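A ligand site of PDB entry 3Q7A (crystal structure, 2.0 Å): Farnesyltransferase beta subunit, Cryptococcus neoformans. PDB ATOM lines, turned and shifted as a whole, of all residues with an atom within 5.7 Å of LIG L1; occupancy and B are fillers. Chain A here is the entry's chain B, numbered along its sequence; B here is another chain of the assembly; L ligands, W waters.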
ATOM      1  N   TRP A  90      26.969 -21.873 -37.384  1.00  0.00           N
ATOM      2  CA  TRP A  90      25.531 -22.003 -37.135  1.00  0.00           C
ATOM      3  C   TRP A  90      24.745 -22.025 -38.433  1.00  0.00           C
ATOM      4  O   TRP A  90      23.800 -22.795 -38.574  1.00  0.00           O
ATOM      5  CB  TRP A  90      25.021 -20.885 -36.221  1.00  0.00           C
ATOM      6  CG  TRP A  90      25.393 -21.078 -34.778  1.00  0.00           C
ATOM      7  CD1 TRP A  90      26.343 -20.389 -34.083  1.00  0.00           C
ATOM      8  CD2 TRP A  90      24.823 -22.026 -33.865  1.00  0.00           C
ATOM      9  NE1 TRP A  90      26.395 -20.852 -32.783  1.00  0.00           N
ATOM     10  CE2 TRP A  90      25.484 -21.852 -32.628  1.00  0.00           C
ATOM     11  CE3 TRP A  90      23.822 -23.009 -33.967  1.00  0.00           C
ATOM     12  CZ2 TRP A  90      25.166 -22.628 -31.501  1.00  0.00           C
ATOM     13  CZ3 TRP A  90      23.517 -23.772 -32.853  1.00  0.00           C
ATOM     14  CH2 TRP A  90      24.190 -23.573 -31.627  1.00  0.00           C
ATOM     15  N   LEU A 141      30.251 -22.041 -28.567  1.00  0.00           N
ATOM     16  CA  LEU A 141      29.037 -22.197 -29.374  1.00  0.00           C
ATOM     17  C   LEU A 141      29.282 -22.704 -30.811  1.00  0.00           C
ATOM     18  O   LEU A 141      28.642 -23.666 -31.231  1.00  0.00           O
ATOM     19  CB  LEU A 141      28.179 -20.924 -29.335  1.00  0.00           C
ATOM     20  CG  LEU A 141      27.239 -20.749 -28.130  1.00  0.00           C
ATOM     21  CD1 LEU A 141      27.957 -20.844 -26.772  1.00  0.00           C
ATOM     22  CD2 LEU A 141      26.469 -19.436 -28.216  1.00  0.00           C
ATOM     23  N   TYR A 144      30.181 -26.420 -30.649  1.00  0.00           N
ATOM     24  CA  TYR A 144      28.992 -27.285 -30.727  1.00  0.00           C
ATOM     25  C   TYR A 144      28.456 -27.372 -32.149  1.00  0.00           C
ATOM     26  O   TYR A 144      28.183 -28.467 -32.653  1.00  0.00           O
ATOM     27  CB  TYR A 144      27.881 -26.803 -29.779  1.00  0.00           C
ATOM     28  CG  TYR A 144      26.511 -27.384 -30.079  1.00  0.00           C
ATOM     29  CD1 TYR A 144      26.069 -28.555 -29.467  1.00  0.00           C
ATOM     30  CD2 TYR A 144      25.637 -26.742 -30.971  1.00  0.00           C
ATOM     31  CE1 TYR A 144      24.805 -29.086 -29.737  1.00  0.00           C
ATOM     32  CE2 TYR A 144      24.375 -27.269 -31.257  1.00  0.00           C
ATOM     33  CZ  TYR A 144      23.970 -28.444 -30.642  1.00  0.00           C
ATOM     34  OH  TYR A 144      22.723 -28.957 -30.917  1.00  0.00           O
ATOM     35  N   ARG A 197      24.335 -21.399 -22.106  1.00  0.00           N
ATOM     36  CA  ARG A 197      24.601 -21.772 -23.509  1.00  0.00           C
ATOM     37  C   ARG A 197      25.989 -22.377 -23.636  1.00  0.00           C
ATOM     38  O   ARG A 197      26.183 -23.384 -24.309  1.00  0.00           O
ATOM     39  CB  ARG A 197      24.498 -20.565 -24.450  1.00  0.00           C
ATOM     40  CG  ARG A 197      23.145 -19.867 -24.524  1.00  0.00           C
ATOM     41  CD  ARG A 197      23.271 -18.557 -25.306  1.00  0.00           C
ATOM     42  NE  ARG A 197      24.374 -17.736 -24.789  1.00  0.00           N
ATOM     43  CZ  ARG A 197      25.103 -16.880 -25.502  1.00  0.00           C
ATOM     44  NH1 ARG A 197      24.859 -16.692 -26.788  1.00  0.00           N
ATOM     45  NH2 ARG A 197      26.081 -16.200 -24.914  1.00  0.00           N
ATOM     46  N   TYR A 200      26.030 -25.883 -21.958  1.00  0.00           N
ATOM     47  CA  TYR A 200      25.362 -26.865 -22.821  1.00  0.00           C
ATOM     48  C   TYR A 200      26.238 -27.288 -23.998  1.00  0.00           C
ATOM     49  O   TYR A 200      26.428 -28.483 -24.227  1.00  0.00           O
ATOM     50  CB  TYR A 200      24.016 -26.335 -23.341  1.00  0.00           C
ATOM     51  CG  TYR A 200      23.478 -27.136 -24.517  1.00  0.00           C
ATOM     52  CD1 TYR A 200      22.941 -28.407 -24.317  1.00  0.00           C
ATOM     53  CD2 TYR A 200      23.534 -26.639 -25.813  1.00  0.00           C
ATOM     54  CE1 TYR A 200      22.455 -29.158 -25.391  1.00  0.00           C
ATOM     55  CE2 TYR A 200      23.052 -27.380 -26.896  1.00  0.00           C
ATOM     56  CZ  TYR A 200      22.505 -28.638 -26.665  1.00  0.00           C
ATOM     57  OH  TYR A 200      22.033 -29.393 -27.714  1.00  0.00           O
ATOM     58  N   CYS A 201      26.765 -26.312 -24.736  1.00  0.00           N
ATOM     59  CA  CYS A 201      27.585 -26.582 -25.906  1.00  0.00           C
ATOM     60  C   CYS A 201      28.832 -27.389 -25.571  1.00  0.00           C
ATOM     61  O   CYS A 201      29.195 -28.311 -26.301  1.00  0.00           O
ATOM     62  CB  CYS A 201      27.944 -25.269 -26.612  1.00  0.00           C
ATOM     63  SG  CYS A 201      26.519 -24.507 -27.426  1.00  0.00           S
ATOM     64  N   HIS A 266      13.874 -18.442 -19.271  1.00  0.00           N
ATOM     65  CA  HIS A 266      13.694 -18.321 -20.709  1.00  0.00           C
ATOM     66  C   HIS A 266      13.802 -19.694 -21.361  1.00  0.00           C
ATOM     67  O   HIS A 266      14.574 -20.539 -20.918  1.00  0.00           O
ATOM     68  CB  HIS A 266      14.740 -17.376 -21.322  1.00  0.00           C
ATOM     69  CG  HIS A 266      14.407 -16.955 -22.718  1.00  0.00           C
ATOM     70  ND1 HIS A 266      13.822 -15.736 -23.002  1.00  0.00           N
ATOM     71  CD2 HIS A 266      14.549 -17.584 -23.898  1.00  0.00           C
ATOM     72  CE1 HIS A 266      13.627 -15.648 -24.306  1.00  0.00           C
ATOM     73  NE2 HIS A 266      14.058 -16.745 -24.872  1.00  0.00           N
ATOM     74  N   GLY A 267      13.021 -19.907 -22.424  1.00  0.00           N
ATOM     75  CA  GLY A 267      13.038 -21.155 -23.194  1.00  0.00           C
ATOM     76  C   GLY A 267      14.430 -21.585 -23.637  1.00  0.00           C
ATOM     77  O   GLY A 267      14.790 -22.757 -23.524  1.00  0.00           O
ATOM     78  N   GLY A 268      15.205 -20.637 -24.149  1.00  0.00           N
ATOM     79  CA  GLY A 268      16.562 -20.919 -24.590  1.00  0.00           C
ATOM     80  C   GLY A 268      17.469 -21.431 -23.484  1.00  0.00           C
ATOM     81  O   GLY A 268      18.163 -22.433 -23.649  1.00  0.00           O
ATOM     82  N   TYR A 269      17.455 -20.724 -22.353  1.00  0.00           N
ATOM     83  CA  TYR A 269      18.278 -21.094 -21.211  1.00  0.00           C
ATOM     84  C   TYR A 269      17.732 -22.286 -20.431  1.00  0.00           C
ATOM     85  O   TYR A 269      18.498 -23.038 -19.823  1.00  0.00           O
ATOM     86  CB  TYR A 269      18.496 -19.887 -20.292  1.00  0.00           C
ATOM     87  CG  TYR A 269      19.195 -18.732 -20.990  1.00  0.00           C
ATOM     88  CD1 TYR A 269      20.452 -18.912 -21.580  1.00  0.00           C
ATOM     89  CD2 TYR A 269      18.613 -17.468 -21.047  1.00  0.00           C
ATOM     90  CE1 TYR A 269      21.102 -17.849 -22.216  1.00  0.00           C
ATOM     91  CE2 TYR A 269      19.254 -16.408 -21.680  1.00  0.00           C
ATOM     92  CZ  TYR A 269      20.495 -16.606 -22.264  1.00  0.00           C
ATOM     93  OH  TYR A 269      21.146 -15.574 -22.890  1.00  0.00           O
ATOM     94  N   CYS A 272      18.914 -25.258 -22.531  1.00  0.00           N
ATOM     95  CA  CYS A 272      20.328 -25.484 -22.253  1.00  0.00           C
ATOM     96  C   CYS A 272      20.566 -26.085 -20.858  1.00  0.00           C
ATOM     97  O   CYS A 272      21.423 -26.953 -20.685  1.00  0.00           O
ATOM     98  CB  CYS A 272      21.132 -24.202 -22.419  1.00  0.00           C
ATOM     99  SG  CYS A 272      21.337 -23.694 -24.137  1.00  0.00           S
ATOM    100  N   GLY A 316       8.726 -17.833 -25.428  1.00  0.00           N
ATOM    101  CA  GLY A 316      10.028 -18.023 -24.789  1.00  0.00           C
ATOM    102  C   GLY A 316      10.080 -17.664 -23.311  1.00  0.00           C
ATOM    103  O   GLY A 316      10.930 -18.157 -22.577  1.00  0.00           O
ATOM    104  N   ARG A 317       9.154 -16.797 -22.900  1.00  0.00           N
ATOM    105  CA  ARG A 317       9.022 -16.401 -21.493  1.00  0.00           C
ATOM    106  C   ARG A 317       7.631 -15.852 -21.219  1.00  0.00           C
ATOM    107  O   ARG A 317       6.938 -15.394 -22.134  1.00  0.00           O
ATOM    108  CB  ARG A 317      10.097 -15.386 -21.076  1.00  0.00           C
ATOM    109  CG  ARG A 317      10.396 -14.301 -22.095  1.00  0.00           C
ATOM    110  CD  ARG A 317      11.488 -13.350 -21.608  1.00  0.00           C
ATOM    111  NE  ARG A 317      12.049 -12.567 -22.704  1.00  0.00           N
ATOM    112  CZ  ARG A 317      12.623 -11.377 -22.554  1.00  0.00           C
ATOM    113  NH1 ARG A 317      12.713 -10.819 -21.358  1.00  0.00           N
ATOM    114  NH2 ARG A 317      13.102 -10.743 -23.613  1.00  0.00           N
ATOM    115  N   LYS A 320       5.346 -12.849 -22.916  1.00  0.00           N
ATOM    116  CA  LYS A 320       5.938 -12.488 -24.194  1.00  0.00           C
ATOM    117  C   LYS A 320       5.204 -13.222 -25.317  1.00  0.00           C
ATOM    118  O   LYS A 320       4.146 -13.820 -25.082  1.00  0.00           O
ATOM    119  CB  LYS A 320       7.431 -12.767 -24.188  1.00  0.00           C
ATOM    120  CG  LYS A 320       8.274 -11.677 -23.517  1.00  0.00           C
ATOM    121  CD  LYS A 320       8.470 -10.509 -24.475  1.00  0.00           C
ATOM    122  CE  LYS A 320       9.896 -10.035 -24.475  1.00  0.00           C
ATOM    123  NZ  LYS A 320      10.255  -9.466 -25.796  1.00  0.00           N
ATOM    124  N   LEU A 321       5.758 -13.187 -26.529  1.00  0.00           N
ATOM    125  CA  LEU A 321       5.044 -13.669 -27.720  1.00  0.00           C
ATOM    126  C   LEU A 321       5.437 -15.074 -28.143  1.00  0.00           C
ATOM    127  O   LEU A 321       6.596 -15.494 -27.983  1.00  0.00           O
ATOM    128  CB  LEU A 321       5.200 -12.686 -28.888  1.00  0.00           C
ATOM    129  CG  LEU A 321       4.749 -11.240 -28.647  1.00  0.00           C
ATOM    130  CD1 LEU A 321       5.093 -10.356 -29.852  1.00  0.00           C
ATOM    131  CD2 LEU A 321       3.258 -11.157 -28.335  1.00  0.00           C
ATOM    132  N   ASP A 323       6.521 -17.947 -30.703  1.00  0.00           N
ATOM    133  CA  ASP A 323       7.577 -17.877 -31.704  1.00  0.00           C
ATOM    134  C   ASP A 323       7.963 -19.295 -32.101  1.00  0.00           C
ATOM    135  O   ASP A 323       8.259 -20.125 -31.238  1.00  0.00           O
ATOM    136  CB  ASP A 323       8.779 -17.110 -31.152  1.00  0.00           C
ATOM    137  CG  ASP A 323       9.960 -17.034 -32.107  1.00  0.00           C
ATOM    138  OD1 ASP A 323      10.058 -17.827 -33.069  1.00  0.00           O
ATOM    139  OD2 ASP A 323      10.827 -16.159 -31.891  1.00  0.00           O
ATOM    140  N   CYS A 325      10.584 -20.718 -33.206  1.00  0.00           N
ATOM    141  CA  CYS A 325      11.869 -21.299 -32.783  1.00  0.00           C
ATOM    142  C   CYS A 325      11.789 -21.988 -31.423  1.00  0.00           C
ATOM    143  O   CYS A 325      12.560 -22.911 -31.154  1.00  0.00           O
ATOM    144  CB  CYS A 325      13.015 -20.272 -32.827  1.00  0.00           C
ATOM    145  SG  CYS A 325      12.951 -18.945 -31.595  1.00  0.00           S
ATOM    146  N   TYR A 326      10.847 -21.565 -30.576  1.00  0.00           N
ATOM    147  CA  TYR A 326      10.670 -22.157 -29.245  1.00  0.00           C
ATOM    148  C   TYR A 326      10.005 -23.531 -29.277  1.00  0.00           C
ATOM    149  O   TYR A 326       9.888 -24.188 -28.241  1.00  0.00           O
ATOM    150  CB  TYR A 326       9.947 -21.188 -28.302  1.00  0.00           C
ATOM    151  CG  TYR A 326      10.724 -19.908 -28.119  1.00  0.00           C
ATOM    152  CD1 TYR A 326      12.057 -19.930 -27.723  1.00  0.00           C
ATOM    153  CD2 TYR A 326      10.129 -18.676 -28.371  1.00  0.00           C
ATOM    154  CE1 TYR A 326      12.792 -18.762 -27.584  1.00  0.00           C
ATOM    155  CE2 TYR A 326      10.854 -17.496 -28.223  1.00  0.00           C
ATOM    156  CZ  TYR A 326      12.182 -17.547 -27.829  1.00  0.00           C
ATOM    157  OH  TYR A 326      12.904 -16.391 -27.676  1.00  0.00           O
ATOM    158  N   TRP A 329      13.278 -25.065 -28.534  1.00  0.00           N
ATOM    159  CA  TRP A 329      13.837 -24.701 -27.228  1.00  0.00           C
ATOM    160  C   TRP A 329      12.950 -25.104 -26.054  1.00  0.00           C
ATOM    161  O   TRP A 329      13.438 -25.655 -25.065  1.00  0.00           O
ATOM    162  CB  TRP A 329      14.212 -23.213 -27.149  1.00  0.00           C
ATOM    163  CG  TRP A 329      15.160 -22.778 -28.237  1.00  0.00           C
ATOM    164  CD1 TRP A 329      14.901 -21.886 -29.224  1.00  0.00           C
ATOM    165  CD2 TRP A 329      16.496 -23.259 -28.453  1.00  0.00           C
ATOM    166  NE1 TRP A 329      15.997 -21.755 -30.050  1.00  0.00           N
ATOM    167  CE2 TRP A 329      16.987 -22.582 -29.601  1.00  0.00           C
ATOM    168  CE3 TRP A 329      17.328 -24.176 -27.793  1.00  0.00           C
ATOM    169  CZ2 TRP A 329      18.277 -22.808 -30.102  1.00  0.00           C
ATOM    170  CZ3 TRP A 329      18.611 -24.399 -28.306  1.00  0.00           C
ATOM    171  CH2 TRP A 329      19.067 -23.712 -29.451  1.00  0.00           C
ATOM    172  N   TYR A 409      17.925 -19.918 -39.041  1.00  0.00           N
ATOM    173  CA  TYR A 409      17.744 -20.189 -37.615  1.00  0.00           C
ATOM    174  C   TYR A 409      16.320 -20.668 -37.299  1.00  0.00           C
ATOM    175  O   TYR A 409      16.143 -21.678 -36.612  1.00  0.00           O
ATOM    176  CB  TYR A 409      18.103 -18.946 -36.784  1.00  0.00           C
ATOM    177  CG  TYR A 409      17.602 -18.979 -35.357  1.00  0.00           C
ATOM    178  CD1 TYR A 409      18.291 -19.689 -34.365  1.00  0.00           C
ATOM    179  CD2 TYR A 409      16.432 -18.313 -34.999  1.00  0.00           C
ATOM    180  CE1 TYR A 409      17.826 -19.729 -33.049  1.00  0.00           C
ATOM    181  CE2 TYR A 409      15.953 -18.353 -33.690  1.00  0.00           C
ATOM    182  CZ  TYR A 409      16.658 -19.060 -32.732  1.00  0.00           C
ATOM    183  OH  TYR A 409      16.180 -19.097 -31.440  1.00  0.00           O
ATOM    184  N   TYR B 123      25.250  -9.601 -27.393  1.00  0.00           N
ATOM    185  CA  TYR B 123      25.845 -10.168 -26.181  1.00  0.00           C
ATOM    186  C   TYR B 123      27.180  -9.475 -25.876  1.00  0.00           C
ATOM    187  O   TYR B 123      27.483  -9.167 -24.715  1.00  0.00           O
ATOM    188  CB  TYR B 123      26.127 -11.660 -26.369  1.00  0.00           C
ATOM    189  CG  TYR B 123      24.960 -12.589 -26.119  1.00  0.00           C
ATOM    190  CD1 TYR B 123      24.686 -13.073 -24.839  1.00  0.00           C
ATOM    191  CD2 TYR B 123      24.142 -13.007 -27.170  1.00  0.00           C
ATOM    192  CE1 TYR B 123      23.610 -13.936 -24.605  1.00  0.00           C
ATOM    193  CE2 TYR B 123      23.073 -13.874 -26.947  1.00  0.00           C
ATOM    194  CZ  TYR B 123      22.817 -14.334 -25.665  1.00  0.00           C
ATOM    195  OH  TYR B 123      21.759 -15.193 -25.440  1.00  0.00           O
ATOM    196  N   LYS B 157      11.717  -4.977 -21.708  1.00  0.00           N
ATOM    197  CA  LYS B 157      11.897  -6.412 -21.464  1.00  0.00           C
ATOM    198  C   LYS B 157      13.210  -6.968 -22.006  1.00  0.00           C
ATOM    199  O   LYS B 157      13.427  -8.186 -21.993  1.00  0.00           O
ATOM    200  CB  LYS B 157      10.709  -7.198 -22.019  1.00  0.00           C
ATOM    201  CG  LYS B 157       9.358  -6.829 -21.413  1.00  0.00           C
ATOM    202  CD  LYS B 157       8.246  -7.687 -21.964  1.00  0.00           C
ATOM    203  CE  LYS B 157       6.904  -7.298 -21.376  1.00  0.00           C
ATOM    204  NZ  LYS B 157       5.862  -8.289 -21.718  1.00  0.00           N
ATOM    205  N   ASN B 158      14.089  -6.082 -22.479  1.00  0.00           N
ATOM    206  CA  ASN B 158      15.383  -6.510 -23.023  1.00  0.00           C
ATOM    207  C   ASN B 158      16.109  -7.413 -22.025  1.00  0.00           C
ATOM    208  O   ASN B 158      16.493  -6.976 -20.937  1.00  0.00           O
ATOM    209  CB  ASN B 158      16.261  -5.310 -23.397  1.00  0.00           C
ATOM    210  CG  ASN B 158      17.561  -5.725 -24.056  1.00  0.00           C
ATOM    211  OD1 ASN B 158      18.493  -6.191 -23.395  1.00  0.00           O
ATOM    212  ND2 ASN B 158      17.641  -5.557 -25.368  1.00  0.00           N
ATOM    213  N   TYR B 159      16.285  -8.678 -22.404  1.00  0.00           N
ATOM    214  CA  TYR B 159      16.806  -9.695 -21.500  1.00  0.00           C
ATOM    215  C   TYR B 159      18.218  -9.382 -21.021  1.00  0.00           C
ATOM    216  O   TYR B 159      18.506  -9.508 -19.823  1.00  0.00           O
ATOM    217  CB  TYR B 159      16.758 -11.087 -22.151  1.00  0.00           C
ATOM    218  CG  TYR B 159      16.944 -12.213 -21.169  1.00  0.00           C
ATOM    219  CD1 TYR B 159      15.841 -12.886 -20.629  1.00  0.00           C
ATOM    220  CD2 TYR B 159      18.220 -12.606 -20.744  1.00  0.00           C
ATOM    221  CE1 TYR B 159      16.007 -13.920 -19.710  1.00  0.00           C
ATOM    222  CE2 TYR B 159      18.394 -13.638 -19.830  1.00  0.00           C
ATOM    223  CZ  TYR B 159      17.283 -14.297 -19.323  1.00  0.00           C
ATOM    224  OH  TYR B 159      17.464 -15.314 -18.411  1.00  0.00           O
ATOM    225  N   HIS B 160      19.082  -8.973 -21.945  1.00  0.00           N
ATOM    226  CA  HIS B 160      20.476  -8.634 -21.623  1.00  0.00           C
ATOM    227  C   HIS B 160      20.552  -7.518 -20.575  1.00  0.00           C
ATOM    228  O   HIS B 160      21.351  -7.597 -19.634  1.00  0.00           O
ATOM    229  CB  HIS B 160      21.239  -8.201 -22.870  1.00  0.00           C
ATOM    230  CG  HIS B 160      21.239  -9.216 -23.969  1.00  0.00           C
ATOM    231  ND1 HIS B 160      21.987 -10.369 -23.919  1.00  0.00           N
ATOM    232  CD2 HIS B 160      20.588  -9.244 -25.163  1.00  0.00           C
ATOM    233  CE1 HIS B 160      21.794 -11.070 -25.025  1.00  0.00           C
ATOM    234  NE2 HIS B 160      20.943 -10.409 -25.796  1.00  0.00           N
HETATM  235  C1  LIG L   1      15.730 -13.141 -25.538  1.00  0.00           C
HETATM  236  O1  LIG L   1      15.614 -12.614 -26.865  1.00  0.00           O
HETATM  237  C2  LIG L   1      16.471 -14.328 -25.539  1.00  0.00           C
HETATM  238  C3  LIG L   1      17.801 -14.532 -25.146  1.00  0.00           C
HETATM  239  C4  LIG L   1      18.651 -13.358 -24.645  1.00  0.00           C
HETATM  240  C5  LIG L   1      18.467 -15.923 -25.187  1.00  0.00           C
HETATM  241  C6  LIG L   1      17.748 -16.966 -26.065  1.00  0.00           C
HETATM  242  C7  LIG L   1      18.438 -18.182 -26.092  1.00  0.00           C
HETATM  243  C8  LIG L   1      18.192 -19.291 -26.907  1.00  0.00           C
HETATM  244  C9  LIG L   1      16.996 -19.305 -27.881  1.00  0.00           C
HETATM  245  C10 LIG L   1      19.003 -20.580 -26.775  1.00  0.00           C
HETATM  246  C11 LIG L   1      20.484 -20.478 -27.134  1.00  0.00           C
HETATM  247  C12 LIG L   1      21.017 -21.769 -27.208  1.00  0.00           C
HETATM  248  C13 LIG L   1      22.239 -22.165 -27.764  1.00  0.00           C
HETATM  249  C14 LIG L   1      23.183 -21.137 -28.381  1.00  0.00           C
HETATM  250  C15 LIG L   1      22.635 -23.640 -27.743  1.00  0.00           C
HETATM  251  P1  LIG L   1      14.313 -11.774 -27.377  1.00  0.00           P
HETATM  252  O2  LIG L   1      13.859 -10.841 -26.327  1.00  0.00           O
HETATM  253  O3  LIG L   1      14.666 -11.254 -28.711  1.00  0.00           O
HETATM  254  O4  LIG L   1      13.225 -12.956 -27.585  1.00  0.00           O
HETATM  255  P2  LIG L   1      11.844 -13.135 -26.731  1.00  0.00           P
HETATM  256  O5  LIG L   1      10.915 -11.990 -26.870  1.00  0.00           O
HETATM  257  O6  LIG L   1      12.231 -13.430 -25.215  1.00  0.00           O
HETATM  258  O7  LIG L   1      11.239 -14.505 -27.293  1.00  0.00           O
HETATM  259  N1  LG2 L   2      18.043 -14.219 -32.375  1.00  0.00           N
HETATM  260  C1  LG2 L   2      18.111 -14.859 -33.704  1.00  0.00           C
HETATM  261  C2  LG2 L   2      16.825 -13.404 -32.244  1.00  0.00           C
HETATM  262  C3  LG2 L   2      19.282 -13.464 -32.138  1.00  0.00           C
HETATM  263  C4  LG2 L   2      19.092 -16.046 -33.641  1.00  0.00           C
HETATM  264  C5  LG2 L   2      15.654 -14.358 -31.922  1.00  0.00           C
HETATM  265  C6  LG2 L   2      20.459 -14.455 -32.185  1.00  0.00           C
HETATM  266  N2  LG2 L   2      20.352 -15.669 -32.914  1.00  0.00           N
HETATM  267  N3  LG2 L   2      15.321 -14.855 -30.742  1.00  0.00           N
HETATM  268  C7  LG2 L   2      14.796 -14.862 -32.801  1.00  0.00           C
HETATM  269  O1  LG2 L   2      21.494 -14.187 -31.587  1.00  0.00           O
HETATM  270  C8  LG2 L   2      21.424 -16.599 -32.934  1.00  0.00           C
HETATM  271  C9  LG2 L   2      15.976 -14.554 -29.458  1.00  0.00           C
HETATM  272  C10 LG2 L   2      14.258 -15.646 -30.853  1.00  0.00           C
HETATM  273  N4  LG2 L   2      13.939 -15.661 -32.155  1.00  0.00           N
HETATM  274  C11 LG2 L   2      21.237 -17.840 -32.328  1.00  0.00           C
HETATM  275  C12 LG2 L   2      22.637 -16.305 -33.547  1.00  0.00           C
HETATM  276  C13 LG2 L   2      17.365 -15.185 -29.304  1.00  0.00           C
HETATM  277  C14 LG2 L   2      22.266 -18.780 -32.326  1.00  0.00           C
HETATM  278  C15 LG2 L   2      23.674 -17.244 -33.549  1.00  0.00           C
HETATM  279  C16 LG2 L   2      18.368 -14.448 -28.663  1.00  0.00           C
HETATM  280  C17 LG2 L   2      17.633 -16.473 -29.761  1.00  0.00           C
HETATM  281  C18 LG2 L   2      23.486 -18.488 -32.926  1.00  0.00           C
HETATM  282 CL1  LG2 L   2      21.995 -20.313 -31.572  1.00  0.00          CL
HETATM  283  C19 LG2 L   2      19.636 -14.987 -28.501  1.00  0.00           C
HETATM  284  C20 LG2 L   2      18.907 -17.014 -29.587  1.00  0.00           C
HETATM  285  C21 LG2 L   2      19.904 -16.275 -28.958  1.00  0.00           C
HETATM  286  C22 LG2 L   2      21.208 -16.835 -28.779  1.00  0.00           C
HETATM  287  N5  LG2 L   2      22.253 -17.283 -28.651  1.00  0.00           N
HETATM  288  O   HOH W   1      13.051 -12.199 -30.799  1.00  0.00           O
HETATM  289  O   HOH W   2       8.300 -12.057 -27.633  1.00  0.00           O
HETATM  290  O   HOH W   3      11.116 -10.738 -29.234  1.00  0.00           O
HETATM  291  O   HOH W   4      15.769  -9.340 -25.086  1.00  0.00           O
HETATM  292  O   HOH W   5      17.260 -10.919 -29.343  1.00  0.00           O
HETATM  293  O   HOH W   6      10.937 -14.170 -30.104  1.00  0.00           O
HETATM  294  O   HOH W   7       8.739 -15.232 -26.301  1.00  0.00           O
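The side-chain hydroxyl of Tyr 326 sits at hydrogen-bond distance from a ring nitrogen (NE2) of His 266.
The guanidinium group (NH1) of Arg 317 lies within hydrogen-bond range of the backbone carbonyl oxygen (O) of Lys 157 of chain B (2.8 Å).
The side-chain sulfur (SG) of Cys 272 is in hydrogen-bond range of the backbone carbonyl oxygen (O) of Gly 268 (3.5 Å).
The side-chain hydroxyl of Tyr 123 of chain B sits at hydrogen-bond distance from the side-chain hydroxyl of Tyr 269.
The side-chain hydroxyl of Tyr 409 lies within hydrogen-bond range of the indole nitrogen of Trp 329 (3.0 Å).
SG of Cys 325 lies close to OH of Tyr 409, at 3.2 Å.
The side-chain hydroxyl of Tyr 200 sits at hydrogen-bond distance from the side-chain hydroxyl of Tyr 144, at 3.3 Å.
The backbone carbonyl oxygen (O) of Arg 197 is in hydrogen-bond range of the side-chain sulfur (SG) of Cys 201 (3.3 Å).
Merely in contact with LIG L1: His 266 (2.8 Å), Gly 268 (3.3 Å), Tyr 123 of chain B (3.4 Å), Trp 329 (3.4 Å), Tyr 269 (3.5 Å), Cys 272 (3.6 Å), Tyr 409 (3.7 Å), Tyr 200 (3.7 Å), Leu 141 (3.7 Å), Arg 197 (3.8 Å), Tyr 159 of chain B (3.9 Å), His 160 of chain B (3.9 Å), Trp 90 (3.99 Å) and Cys 201 (3.99 Å).
Hydrophobic or aromatic side chains that line LIG L1: Trp 90, Leu 141, Tyr 200, His 266, Tyr 269, Tyr 326, Trp 329, Tyr 159 of chain B and His 160 of chain B.
17 residues have an atom within 4 Å of LIG L1: Trp 90, Leu 141, Arg 197, Tyr 200, Cys 201, His 266, Gly 268, Tyr 269, Cys 272, Arg 317, Lys 320, Tyr 326, Trp 329, Tyr 409, Tyr 123 of chain B, Tyr 159 of chain B and His 160 of chain B.
Along chain A the residues within 4 Å of LIG L1 span positions 90 to 409.
OH of Tyr 326 lies within hydrogen-bond range of O7 of LIG L1 (2.5 Å).
NE of Arg 317 is in salt-bridge range of O6 of LIG L1 (2.7 Å).
NZ of Lys 320 lies within salt-bridge range of O5 of LIG L1 (2.8 Å).
A nitrogen (N5) of LG2 L2 is in hydrogen-bond range of the guanidinium group of Arg 197, 3.3 Å away.
Water W2 lies within hydrogen-bond range of O5 of LIG L1 and N of Leu 321.
Water W4 lies within hydrogen-bond range of an oxygen (O2) of LIG L1 (2.7 Å), the backbone NH of Tyr 159 of chain B (2.8 Å) and the guanidinium group of Arg 317 (3.4 Å).
Water W7 lies within hydrogen-bond range of the backbone carbonyl oxygen (O) of Leu 321 (2.7 Å), the backbone NH (N) of Gly 316 (2.7 Å) and an oxygen (O7) of LIG L1 (2.8 Å).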
